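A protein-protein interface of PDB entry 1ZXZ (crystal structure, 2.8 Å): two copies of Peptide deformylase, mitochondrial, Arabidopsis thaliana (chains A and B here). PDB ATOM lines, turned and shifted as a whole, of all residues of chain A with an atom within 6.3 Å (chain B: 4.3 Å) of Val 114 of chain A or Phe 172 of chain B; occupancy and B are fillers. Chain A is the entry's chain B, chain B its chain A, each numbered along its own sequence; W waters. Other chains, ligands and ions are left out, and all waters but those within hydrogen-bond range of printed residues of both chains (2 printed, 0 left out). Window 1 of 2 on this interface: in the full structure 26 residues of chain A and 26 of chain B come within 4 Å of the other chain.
The backbone NH (N) of Arg 170 of chain B lies within hydrogen-bond range of the side-chain carboxylate (OD2) of Asp 165 of chain A, 2.9 Å away.
N of Ser 9 of chain A is in hydrogen-bond range of O of Ser 113 of chain A (2.8 Å).
O of Arg 173 of chain B is in hydrogen-bond range of N of Arg 118 of chain B (2.6 Å).
The backbone carbonyl oxygen (O) of Thr 171 of chain B sits at hydrogen-bond distance from the guanidinium group (NE) of Arg 173 of chain B, 2.8 Å away.
The backbone carbonyl oxygen (O) of Phe 117 of chain A lies within hydrogen-bond range of the side-chain hydroxyl (OH) of Tyr 163 of chain A, 3.4 Å away.
Among the printed residues, pairs that only touch across the chains: Phe 117 of chain A with Phe 117 of chain B (3.0 Å), Gly 10 of chain A with Arg 173 of chain B (3.3 Å), His 15 of chain A with Arg 170 of chain B (3.5 Å), Ser 9 of chain A with Arg 173 of chain B (3.5 Å), Asp 115 of chain A with Phe 117 of chain B (3.6 Å), Ser 9 of chain A with Phe 172 of chain B (3.7 Å), Val 164 of chain A with Met 167 of chain B (3.7 Å), Val 114 of chain A with Phe 117 of chain B (3.8 Å), Asp 165 of chain A with Met 167 of chain B (3.9 Å), Val 114 of chain A with Phe 172 of chain B (3.9 Å), Gly 10 of chain A with Phe 172 of chain B (3.96 Å) and His 15 of chain A with Phe 172 of chain B (3.96 Å).
Of the printed residues of chain B, Ser 9 of chain A touches Phe 172 (3.7 Å) and Arg 173 (3.5 Å).
Of the printed residues of chain B, Phe 117 of chain A touches Phe 117.
Printed residues of chain B within 4 Å of Asp 165 of chain A: Met 167 (3.9 Å) and Arg 170 (2.9 Å).
Arg 118 of chain B touches none of the printed residues of chain A.
Phe 172 of chain B touches just these residues of chain A: Ser 9, Gly 10, His 15 and Val 114.
Hydrophobic or aromatic side chains of chain B within 4 Å of the printed part of chain A: Phe 117, Met 167 and Phe 172.
Of the 20 printed residues of chain A, 8 touch a printed residue of chain B.
Printed residues of chain A that touch a printed residue of chain B: Ser 9, Gly 10, His 15, Val 114, Asp 115, Phe 117, Val 164 and Asp 165.
Hydrophobic or aromatic side chains of chain A that line the printed part of chain B: His 15, Val 114, Phe 117 and Val 164.
Among the printed residues, no Asp or Glu carboxylate lies within 4 Å of a Lys or Arg side-chain nitrogen of the other chain.
Phe 117 of chain A touches its own counterpart, Phe 117 of chain B.
Positions printed for both chains: 117, 118, 164 and 172.
Of the 13 pairs that touch across the chains among the printed residues, 1 has its exchanged pair printed and touching as well.
Water W1 lies within hydrogen-bond range of the backbone carbonyl oxygen (O) of Met 167 of chain B and the side-chain carboxylate (OD1) of Asp 165 of chain A.
Water W2 lies within hydrogen-bond range of NH2 of Arg 173 of chain B (2.8 Å) and O of Gly 10 of chain A (2.8 Å).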
ATOM      1  N   VAL A   7      17.278  -0.750   8.463  1.00  0.00           N
ATOM      2  CA  VAL A   7      18.125   0.014   9.366  1.00  0.00           C
ATOM      3  C   VAL A   7      17.473   0.122  10.738  1.00  0.00           C
ATOM      4  O   VAL A   7      16.296   0.448  10.846  1.00  0.00           O
ATOM      5  CB  VAL A   7      18.403   1.412   8.802  1.00  0.00           C
ATOM      6  CG1 VAL A   7      18.812   1.300   7.356  1.00  0.00           C
ATOM      7  CG2 VAL A   7      17.186   2.281   8.927  1.00  0.00           C
ATOM      8  N   ALA A   8      18.240  -0.163  11.784  1.00  0.00           N
ATOM      9  CA  ALA A   8      17.727  -0.117  13.147  1.00  0.00           C
ATOM     10  C   ALA A   8      17.822   1.289  13.699  1.00  0.00           C
ATOM     11  O   ALA A   8      18.692   2.063  13.291  1.00  0.00           O
ATOM     12  CB  ALA A   8      18.519  -1.069  14.030  1.00  0.00           C
ATOM     13  N   SER A   9      16.929   1.617  14.630  1.00  0.00           N
ATOM     14  CA  SER A   9      16.921   2.939  15.252  1.00  0.00           C
ATOM     15  C   SER A   9      18.338   3.366  15.592  1.00  0.00           C
ATOM     16  O   SER A   9      19.113   2.587  16.143  1.00  0.00           O
ATOM     17  CB  SER A   9      16.088   2.925  16.531  1.00  0.00           C
ATOM     18  OG  SER A   9      14.988   3.802  16.413  1.00  0.00           O
ATOM     19  N   GLY A  10      18.672   4.607  15.264  1.00  0.00           N
ATOM     20  CA  GLY A  10      20.008   5.092  15.543  1.00  0.00           C
ATOM     21  C   GLY A  10      20.568   5.717  14.292  1.00  0.00           C
ATOM     22  O   GLY A  10      21.061   6.844  14.318  1.00  0.00           O
ATOM     23  N   HIS A  15      15.965   9.300  11.140  1.00  0.00           N
ATOM     24  CA  HIS A  15      15.412  10.450  11.850  1.00  0.00           C
ATOM     25  C   HIS A  15      15.505  11.798  11.147  1.00  0.00           C
ATOM     26  O   HIS A  15      15.469  12.844  11.794  1.00  0.00           O
ATOM     27  CB  HIS A  15      16.076  10.544  13.225  1.00  0.00           C
ATOM     28  CG  HIS A  15      16.236   9.215  13.905  1.00  0.00           C
ATOM     29  ND1 HIS A  15      17.315   8.388  13.675  1.00  0.00           N
ATOM     30  CD2 HIS A  15      15.435   8.563  14.779  1.00  0.00           C
ATOM     31  CE1 HIS A  15      17.172   7.281  14.385  1.00  0.00           C
ATOM     32  NE2 HIS A  15      16.043   7.360  15.061  1.00  0.00           N
ATOM     33  N   GLN A  54      13.763   3.202   5.822  1.00  0.00           N
ATOM     34  CA  GLN A  54      14.024   1.949   6.518  1.00  0.00           C
ATOM     35  C   GLN A  54      14.989   0.994   5.814  1.00  0.00           C
ATOM     36  O   GLN A  54      15.321  -0.064   6.349  1.00  0.00           O
ATOM     37  CB  GLN A  54      12.704   1.247   6.845  1.00  0.00           C
ATOM     38  CG  GLN A  54      11.932   1.938   7.964  1.00  0.00           C
ATOM     39  CD  GLN A  54      10.809   1.094   8.530  1.00  0.00           C
ATOM     40  OE1 GLN A  54       9.736   0.981   7.938  1.00  0.00           O
ATOM     41  NE2 GLN A  54      11.055   0.490   9.685  1.00  0.00           N
ATOM     42  N   GLY A 110       4.436  -1.567  16.679  1.00  0.00           N
ATOM     43  CA  GLY A 110       5.821  -1.983  16.639  1.00  0.00           C
ATOM     44  C   GLY A 110       6.433  -1.481  15.340  1.00  0.00           C
ATOM     45  O   GLY A 110       5.728  -1.059  14.427  1.00  0.00           O
ATOM     46  N   CYS A 111       7.751  -1.517  15.257  1.00  0.00           N
ATOM     47  CA  CYS A 111       8.439  -1.081  14.062  1.00  0.00           C
ATOM     48  C   CYS A 111       9.616  -2.009  13.841  1.00  0.00           C
ATOM     49  O   CYS A 111      10.331  -2.338  14.781  1.00  0.00           O
ATOM     50  CB  CYS A 111       8.935   0.342  14.244  1.00  0.00           C
ATOM     51  SG  CYS A 111      10.042   0.868  12.948  1.00  0.00           S
ATOM     52  N   LEU A 112       9.824  -2.445  12.609  1.00  0.00           N
ATOM     53  CA  LEU A 112      10.936  -3.331  12.347  1.00  0.00           C
ATOM     54  C   LEU A 112      12.280  -2.647  12.613  1.00  0.00           C
ATOM     55  O   LEU A 112      13.320  -3.311  12.677  1.00  0.00           O
ATOM     56  CB  LEU A 112      10.863  -3.855  10.917  1.00  0.00           C
ATOM     57  CG  LEU A 112       9.567  -4.644  10.743  1.00  0.00           C
ATOM     58  CD1 LEU A 112       8.476  -3.663  10.353  1.00  0.00           C
ATOM     59  CD2 LEU A 112       9.715  -5.759   9.698  1.00  0.00           C
ATOM     60  N   SER A 113      12.262  -1.328  12.777  1.00  0.00           N
ATOM     61  CA  SER A 113      13.486  -0.594  13.057  1.00  0.00           C
ATOM     62  C   SER A 113      13.716  -0.554  14.567  1.00  0.00           C
ATOM     63  O   SER A 113      14.729  -0.025  15.047  1.00  0.00           O
ATOM     64  CB  SER A 113      13.401   0.831  12.502  1.00  0.00           C
ATOM     65  OG  SER A 113      13.546   0.859  11.094  1.00  0.00           O
ATOM     66  N   VAL A 114      12.770  -1.120  15.310  1.00  0.00           N
ATOM     67  CA  VAL A 114      12.839  -1.162  16.772  1.00  0.00           C
ATOM     68  C   VAL A 114      12.229  -2.481  17.245  1.00  0.00           C
ATOM     69  O   VAL A 114      11.091  -2.502  17.731  1.00  0.00           O
ATOM     70  CB  VAL A 114      12.023  -0.006  17.412  1.00  0.00           C
ATOM     71  CG1 VAL A 114      12.184  -0.026  18.928  1.00  0.00           C
ATOM     72  CG2 VAL A 114      12.456   1.324  16.836  1.00  0.00           C
ATOM     73  N   ASP A 115      12.976  -3.575  17.123  1.00  0.00           N
ATOM     74  CA  ASP A 115      12.411  -4.852  17.517  1.00  0.00           C
ATOM     75  C   ASP A 115      12.605  -5.275  18.959  1.00  0.00           C
ATOM     76  O   ASP A 115      13.489  -4.779  19.664  1.00  0.00           O
ATOM     77  CB  ASP A 115      12.898  -5.966  16.590  1.00  0.00           C
ATOM     78  CG  ASP A 115      14.356  -6.256  16.751  1.00  0.00           C
ATOM     79  OD1 ASP A 115      15.159  -5.320  16.563  1.00  0.00           O
ATOM     80  OD2 ASP A 115      14.683  -7.422  17.061  1.00  0.00           O
ATOM     81  N   GLY A 116      11.746  -6.205  19.374  1.00  0.00           N
ATOM     82  CA  GLY A 116      11.764  -6.736  20.723  1.00  0.00           C
ATOM     83  C   GLY A 116      10.877  -5.929  21.646  1.00  0.00           C
ATOM     84  O   GLY A 116      10.714  -6.288  22.816  1.00  0.00           O
ATOM     85  N   PHE A 117      10.302  -4.845  21.120  1.00  0.00           N
ATOM     86  CA  PHE A 117       9.447  -3.965  21.911  1.00  0.00           C
ATOM     87  C   PHE A 117       8.192  -3.508  21.190  1.00  0.00           C
ATOM     88  O   PHE A 117       8.069  -3.630  19.968  1.00  0.00           O
ATOM     89  CB  PHE A 117      10.229  -2.721  22.349  1.00  0.00           C
ATOM     90  CG  PHE A 117      11.501  -3.029  23.074  1.00  0.00           C
ATOM     91  CD1 PHE A 117      11.556  -2.992  24.460  1.00  0.00           C
ATOM     92  CD2 PHE A 117      12.638  -3.430  22.369  1.00  0.00           C
ATOM     93  CE1 PHE A 117      12.735  -3.329  25.131  1.00  0.00           C
ATOM     94  CE2 PHE A 117      13.812  -3.768  23.031  1.00  0.00           C
ATOM     95  CZ  PHE A 117      13.862  -3.729  24.410  1.00  0.00           C
ATOM     96  N   ARG A 118       7.273  -2.961  21.979  1.00  0.00           N
ATOM     97  CA  ARG A 118       6.009  -2.445  21.499  1.00  0.00           C
ATOM     98  C   ARG A 118       5.601  -1.330  22.439  1.00  0.00           C
ATOM     99  O   ARG A 118       6.219  -1.122  23.483  1.00  0.00           O
ATOM    100  CB  ARG A 118       4.946  -3.531  21.538  1.00  0.00           C
ATOM    101  CG  ARG A 118       5.230  -4.708  20.643  1.00  0.00           C
ATOM    102  CD  ARG A 118       4.946  -4.361  19.192  1.00  0.00           C
ATOM    103  NE  ARG A 118       4.589  -5.545  18.420  1.00  0.00           N
ATOM    104  CZ  ARG A 118       5.464  -6.439  17.975  1.00  0.00           C
ATOM    105  NH1 ARG A 118       6.757  -6.272  18.225  1.00  0.00           N
ATOM    106  NH2 ARG A 118       5.044  -7.506  17.303  1.00  0.00           N
ATOM    107  N   LEU A 162       9.333   8.272  14.833  1.00  0.00           N
ATOM    108  CA  LEU A 162       9.072   6.899  15.232  1.00  0.00           C
ATOM    109  C   LEU A 162       8.015   6.866  16.318  1.00  0.00           C
ATOM    110  O   LEU A 162       7.821   7.847  17.031  1.00  0.00           O
ATOM    111  CB  LEU A 162      10.357   6.243  15.736  1.00  0.00           C
ATOM    112  CG  LEU A 162      11.474   6.028  14.712  1.00  0.00           C
ATOM    113  CD1 LEU A 162      12.555   5.164  15.331  1.00  0.00           C
ATOM    114  CD2 LEU A 162      10.931   5.341  13.480  1.00  0.00           C
ATOM    115  N   TYR A 163       7.330   5.740  16.458  1.00  0.00           N
ATOM    116  CA  TYR A 163       6.298   5.656  17.477  1.00  0.00           C
ATOM    117  C   TYR A 163       6.823   5.987  18.877  1.00  0.00           C
ATOM    118  O   TYR A 163       6.167   6.693  19.636  1.00  0.00           O
ATOM    119  CB  TYR A 163       5.630   4.270  17.444  1.00  0.00           C
ATOM    120  CG  TYR A 163       6.439   3.105  17.973  1.00  0.00           C
ATOM    121  CD1 TYR A 163       6.167   2.568  19.228  1.00  0.00           C
ATOM    122  CD2 TYR A 163       7.414   2.484  17.191  1.00  0.00           C
ATOM    123  CE1 TYR A 163       6.835   1.435  19.684  1.00  0.00           C
ATOM    124  CE2 TYR A 163       8.090   1.350  17.645  1.00  0.00           C
ATOM    125  CZ  TYR A 163       7.792   0.830  18.883  1.00  0.00           C
ATOM    126  OH  TYR A 163       8.438  -0.315  19.282  1.00  0.00           O
ATOM    127  N   VAL A 164       8.017   5.505  19.203  1.00  0.00           N
ATOM    128  CA  VAL A 164       8.600   5.744  20.518  1.00  0.00           C
ATOM    129  C   VAL A 164       8.568   7.209  20.976  1.00  0.00           C
ATOM    130  O   VAL A 164       8.561   7.488  22.176  1.00  0.00           O
ATOM    131  CB  VAL A 164      10.057   5.209  20.582  1.00  0.00           C
ATOM    132  CG1 VAL A 164      10.067   3.732  20.253  1.00  0.00           C
ATOM    133  CG2 VAL A 164      10.948   5.964  19.618  1.00  0.00           C
ATOM    134  N   ASP A 165       8.546   8.143  20.033  1.00  0.00           N
ATOM    135  CA  ASP A 165       8.506   9.557  20.396  1.00  0.00           C
ATOM    136  C   ASP A 165       7.078  10.044  20.320  1.00  0.00           C
ATOM    137  O   ASP A 165       6.818  11.237  20.384  1.00  0.00           O
ATOM    138  CB  ASP A 165       9.358  10.399  19.444  1.00  0.00           C
ATOM    139  CG  ASP A 165      10.823  10.060  19.522  1.00  0.00           C
ATOM    140  OD1 ASP A 165      11.352  10.001  20.649  1.00  0.00           O
ATOM    141  OD2 ASP A 165      11.449   9.864  18.458  1.00  0.00           O
ATOM    142  N   PHE A 172       5.079   1.372  26.900  1.00  0.00           N
ATOM    143  CA  PHE A 172       6.225   0.846  26.164  1.00  0.00           C
ATOM    144  C   PHE A 172       6.662  -0.448  26.835  1.00  0.00           C
ATOM    145  O   PHE A 172       6.998  -0.462  28.019  1.00  0.00           O
ATOM    146  CB  PHE A 172       7.368   1.876  26.165  1.00  0.00           C
ATOM    147  CG  PHE A 172       8.688   1.332  25.686  1.00  0.00           C
ATOM    148  CD1 PHE A 172       9.527   0.656  26.568  1.00  0.00           C
ATOM    149  CD2 PHE A 172       9.099   1.498  24.356  1.00  0.00           C
ATOM    150  CE1 PHE A 172      10.756   0.151  26.146  1.00  0.00           C
ATOM    151  CE2 PHE A 172      10.338   0.992  23.919  1.00  0.00           C
ATOM    152  CZ  PHE A 172      11.166   0.319  24.820  1.00  0.00           C
ATOM    153  N   PHE B 117      18.940  -1.004  23.770  1.00  0.00           N
ATOM    154  CA  PHE B 117      18.702   0.379  23.363  1.00  0.00           C
ATOM    155  C   PHE B 117      19.233   1.466  24.285  1.00  0.00           C
ATOM    156  O   PHE B 117      19.560   1.227  25.446  1.00  0.00           O
ATOM    157  CB  PHE B 117      17.198   0.594  23.173  1.00  0.00           C
ATOM    158  CG  PHE B 117      16.605  -0.265  22.105  1.00  0.00           C
ATOM    159  CD1 PHE B 117      16.314   0.263  20.852  1.00  0.00           C
ATOM    160  CD2 PHE B 117      16.375  -1.618  22.329  1.00  0.00           C
ATOM    161  CE1 PHE B 117      15.807  -0.545  19.831  1.00  0.00           C
ATOM    162  CE2 PHE B 117      15.874  -2.428  21.314  1.00  0.00           C
ATOM    163  CZ  PHE B 117      15.586  -1.890  20.066  1.00  0.00           C
ATOM    164  N   ARG B 118      19.291   2.674  23.740  1.00  0.00           N
ATOM    165  CA  ARG B 118      19.745   3.843  24.467  1.00  0.00           C
ATOM    166  C   ARG B 118      19.013   5.046  23.924  1.00  0.00           C
ATOM    167  O   ARG B 118      18.366   4.964  22.880  1.00  0.00           O
ATOM    168  CB  ARG B 118      21.239   4.045  24.276  1.00  0.00           C
ATOM    169  CG  ARG B 118      22.089   2.956  24.876  1.00  0.00           C
ATOM    170  CD  ARG B 118      22.258   3.095  26.380  1.00  0.00           C
ATOM    171  NE  ARG B 118      23.417   2.308  26.776  1.00  0.00           N
ATOM    172  CZ  ARG B 118      23.413   0.990  26.927  1.00  0.00           C
ATOM    173  NH1 ARG B 118      22.293   0.312  26.718  1.00  0.00           N
ATOM    174  NH2 ARG B 118      24.523   0.352  27.266  1.00  0.00           N
ATOM    175  N   ALA B 119      19.125   6.159  24.641  1.00  0.00           N
ATOM    176  CA  ALA B 119      18.485   7.413  24.256  1.00  0.00           C
ATOM    177  C   ALA B 119      19.029   8.544  25.105  1.00  0.00           C
ATOM    178  O   ALA B 119      19.256   8.397  26.302  1.00  0.00           O
ATOM    179  CB  ALA B 119      16.968   7.321  24.429  1.00  0.00           C
ATOM    180  N   VAL B 164      12.683   6.280  28.531  1.00  0.00           N
ATOM    181  CA  VAL B 164      11.992   6.322  27.250  1.00  0.00           C
ATOM    182  C   VAL B 164      10.829   7.317  27.215  1.00  0.00           C
ATOM    183  O   VAL B 164      10.474   7.831  26.152  1.00  0.00           O
ATOM    184  CB  VAL B 164      11.456   4.923  26.871  1.00  0.00           C
ATOM    185  CG1 VAL B 164      12.612   4.006  26.536  1.00  0.00           C
ATOM    186  CG2 VAL B 164      10.640   4.337  28.028  1.00  0.00           C
ATOM    187  N   MET B 167      12.764  10.963  27.105  1.00  0.00           N
ATOM    188  CA  MET B 167      13.910  11.119  26.219  1.00  0.00           C
ATOM    189  C   MET B 167      13.748  12.134  25.104  1.00  0.00           C
ATOM    190  O   MET B 167      12.633  12.480  24.713  1.00  0.00           O
ATOM    191  CB  MET B 167      14.258   9.773  25.608  1.00  0.00           C
ATOM    192  CG  MET B 167      13.201   9.266  24.648  1.00  0.00           C
ATOM    193  SD  MET B 167      13.559   7.604  24.132  1.00  0.00           S
ATOM    194  CE  MET B 167      12.110   7.209  23.233  1.00  0.00           C
ATOM    195  N   ARG B 170      13.830  11.484  18.609  1.00  0.00           N
ATOM    196  CA  ARG B 170      14.722  10.868  17.637  1.00  0.00           C
ATOM    197  C   ARG B 170      16.177  10.674  18.035  1.00  0.00           C
ATOM    198  O   ARG B 170      17.094  10.933  17.246  1.00  0.00           O
ATOM    199  CB  ARG B 170      14.652  11.622  16.299  1.00  0.00           C
ATOM    200  CG  ARG B 170      13.818  12.899  16.293  1.00  0.00           C
ATOM    201  CD  ARG B 170      13.580  13.371  14.874  1.00  0.00           C
ATOM    202  NE  ARG B 170      13.313  14.797  14.826  1.00  0.00           N
ATOM    203  CZ  ARG B 170      12.277  15.333  14.199  1.00  0.00           C
ATOM    204  NH1 ARG B 170      11.409  14.551  13.577  1.00  0.00           N
ATOM    205  NH2 ARG B 170      12.124  16.650  14.172  1.00  0.00           N
ATOM    206  N   THR B 171      16.394  10.208  19.258  1.00  0.00           N
ATOM    207  CA  THR B 171      17.745   9.938  19.717  1.00  0.00           C
ATOM    208  C   THR B 171      17.782   8.483  20.120  1.00  0.00           C
ATOM    209  O   THR B 171      18.842   7.857  20.142  1.00  0.00           O
ATOM    210  CB  THR B 171      18.141  10.800  20.923  1.00  0.00           C
ATOM    211  OG1 THR B 171      17.215  10.594  21.994  1.00  0.00           O
ATOM    212  CG2 THR B 171      18.158  12.255  20.537  1.00  0.00           C
ATOM    213  N   PHE B 172      16.600   7.959  20.430  1.00  0.00           N
ATOM    214  CA  PHE B 172      16.442   6.565  20.833  1.00  0.00           C
ATOM    215  C   PHE B 172      17.174   5.715  19.819  1.00  0.00           C
ATOM    216  O   PHE B 172      17.012   5.901  18.614  1.00  0.00           O
ATOM    217  CB  PHE B 172      14.962   6.196  20.851  1.00  0.00           C
ATOM    218  CG  PHE B 172      14.671   4.866  21.474  1.00  0.00           C
ATOM    219  CD1 PHE B 172      14.311   3.771  20.683  1.00  0.00           C
ATOM    220  CD2 PHE B 172      14.732   4.712  22.854  1.00  0.00           C
ATOM    221  CE1 PHE B 172      13.999   2.544  21.265  1.00  0.00           C
ATOM    222  CE2 PHE B 172      14.425   3.492  23.451  1.00  0.00           C
ATOM    223  CZ  PHE B 172      14.059   2.401  22.655  1.00  0.00           C
ATOM    224  N   ARG B 173      17.985   4.784  20.293  1.00  0.00           N
ATOM    225  CA  ARG B 173      18.733   3.968  19.358  1.00  0.00           C
ATOM    226  C   ARG B 173      19.245   2.666  19.935  1.00  0.00           C
ATOM    227  O   ARG B 173      19.203   2.425  21.140  1.00  0.00           O
ATOM    228  CB  ARG B 173      19.913   4.778  18.802  1.00  0.00           C
ATOM    229  CG  ARG B 173      20.857   5.339  19.883  1.00  0.00           C
ATOM    230  CD  ARG B 173      21.772   6.393  19.311  1.00  0.00           C
ATOM    231  NE  ARG B 173      21.017   7.325  18.477  1.00  0.00           N
ATOM    232  CZ  ARG B 173      21.560   8.269  17.716  1.00  0.00           C
ATOM    233  NH1 ARG B 173      22.880   8.391  17.648  1.00  0.00           N
ATOM    234  NH2 ARG B 173      20.781   9.170  17.122  1.00  0.00           N
HETATM  235  O   HOH W   1      10.956  11.472  23.013  1.00  0.00           O
HETATM  236  O   HOH W   2      21.068   9.634  14.404  1.00  0.00           O
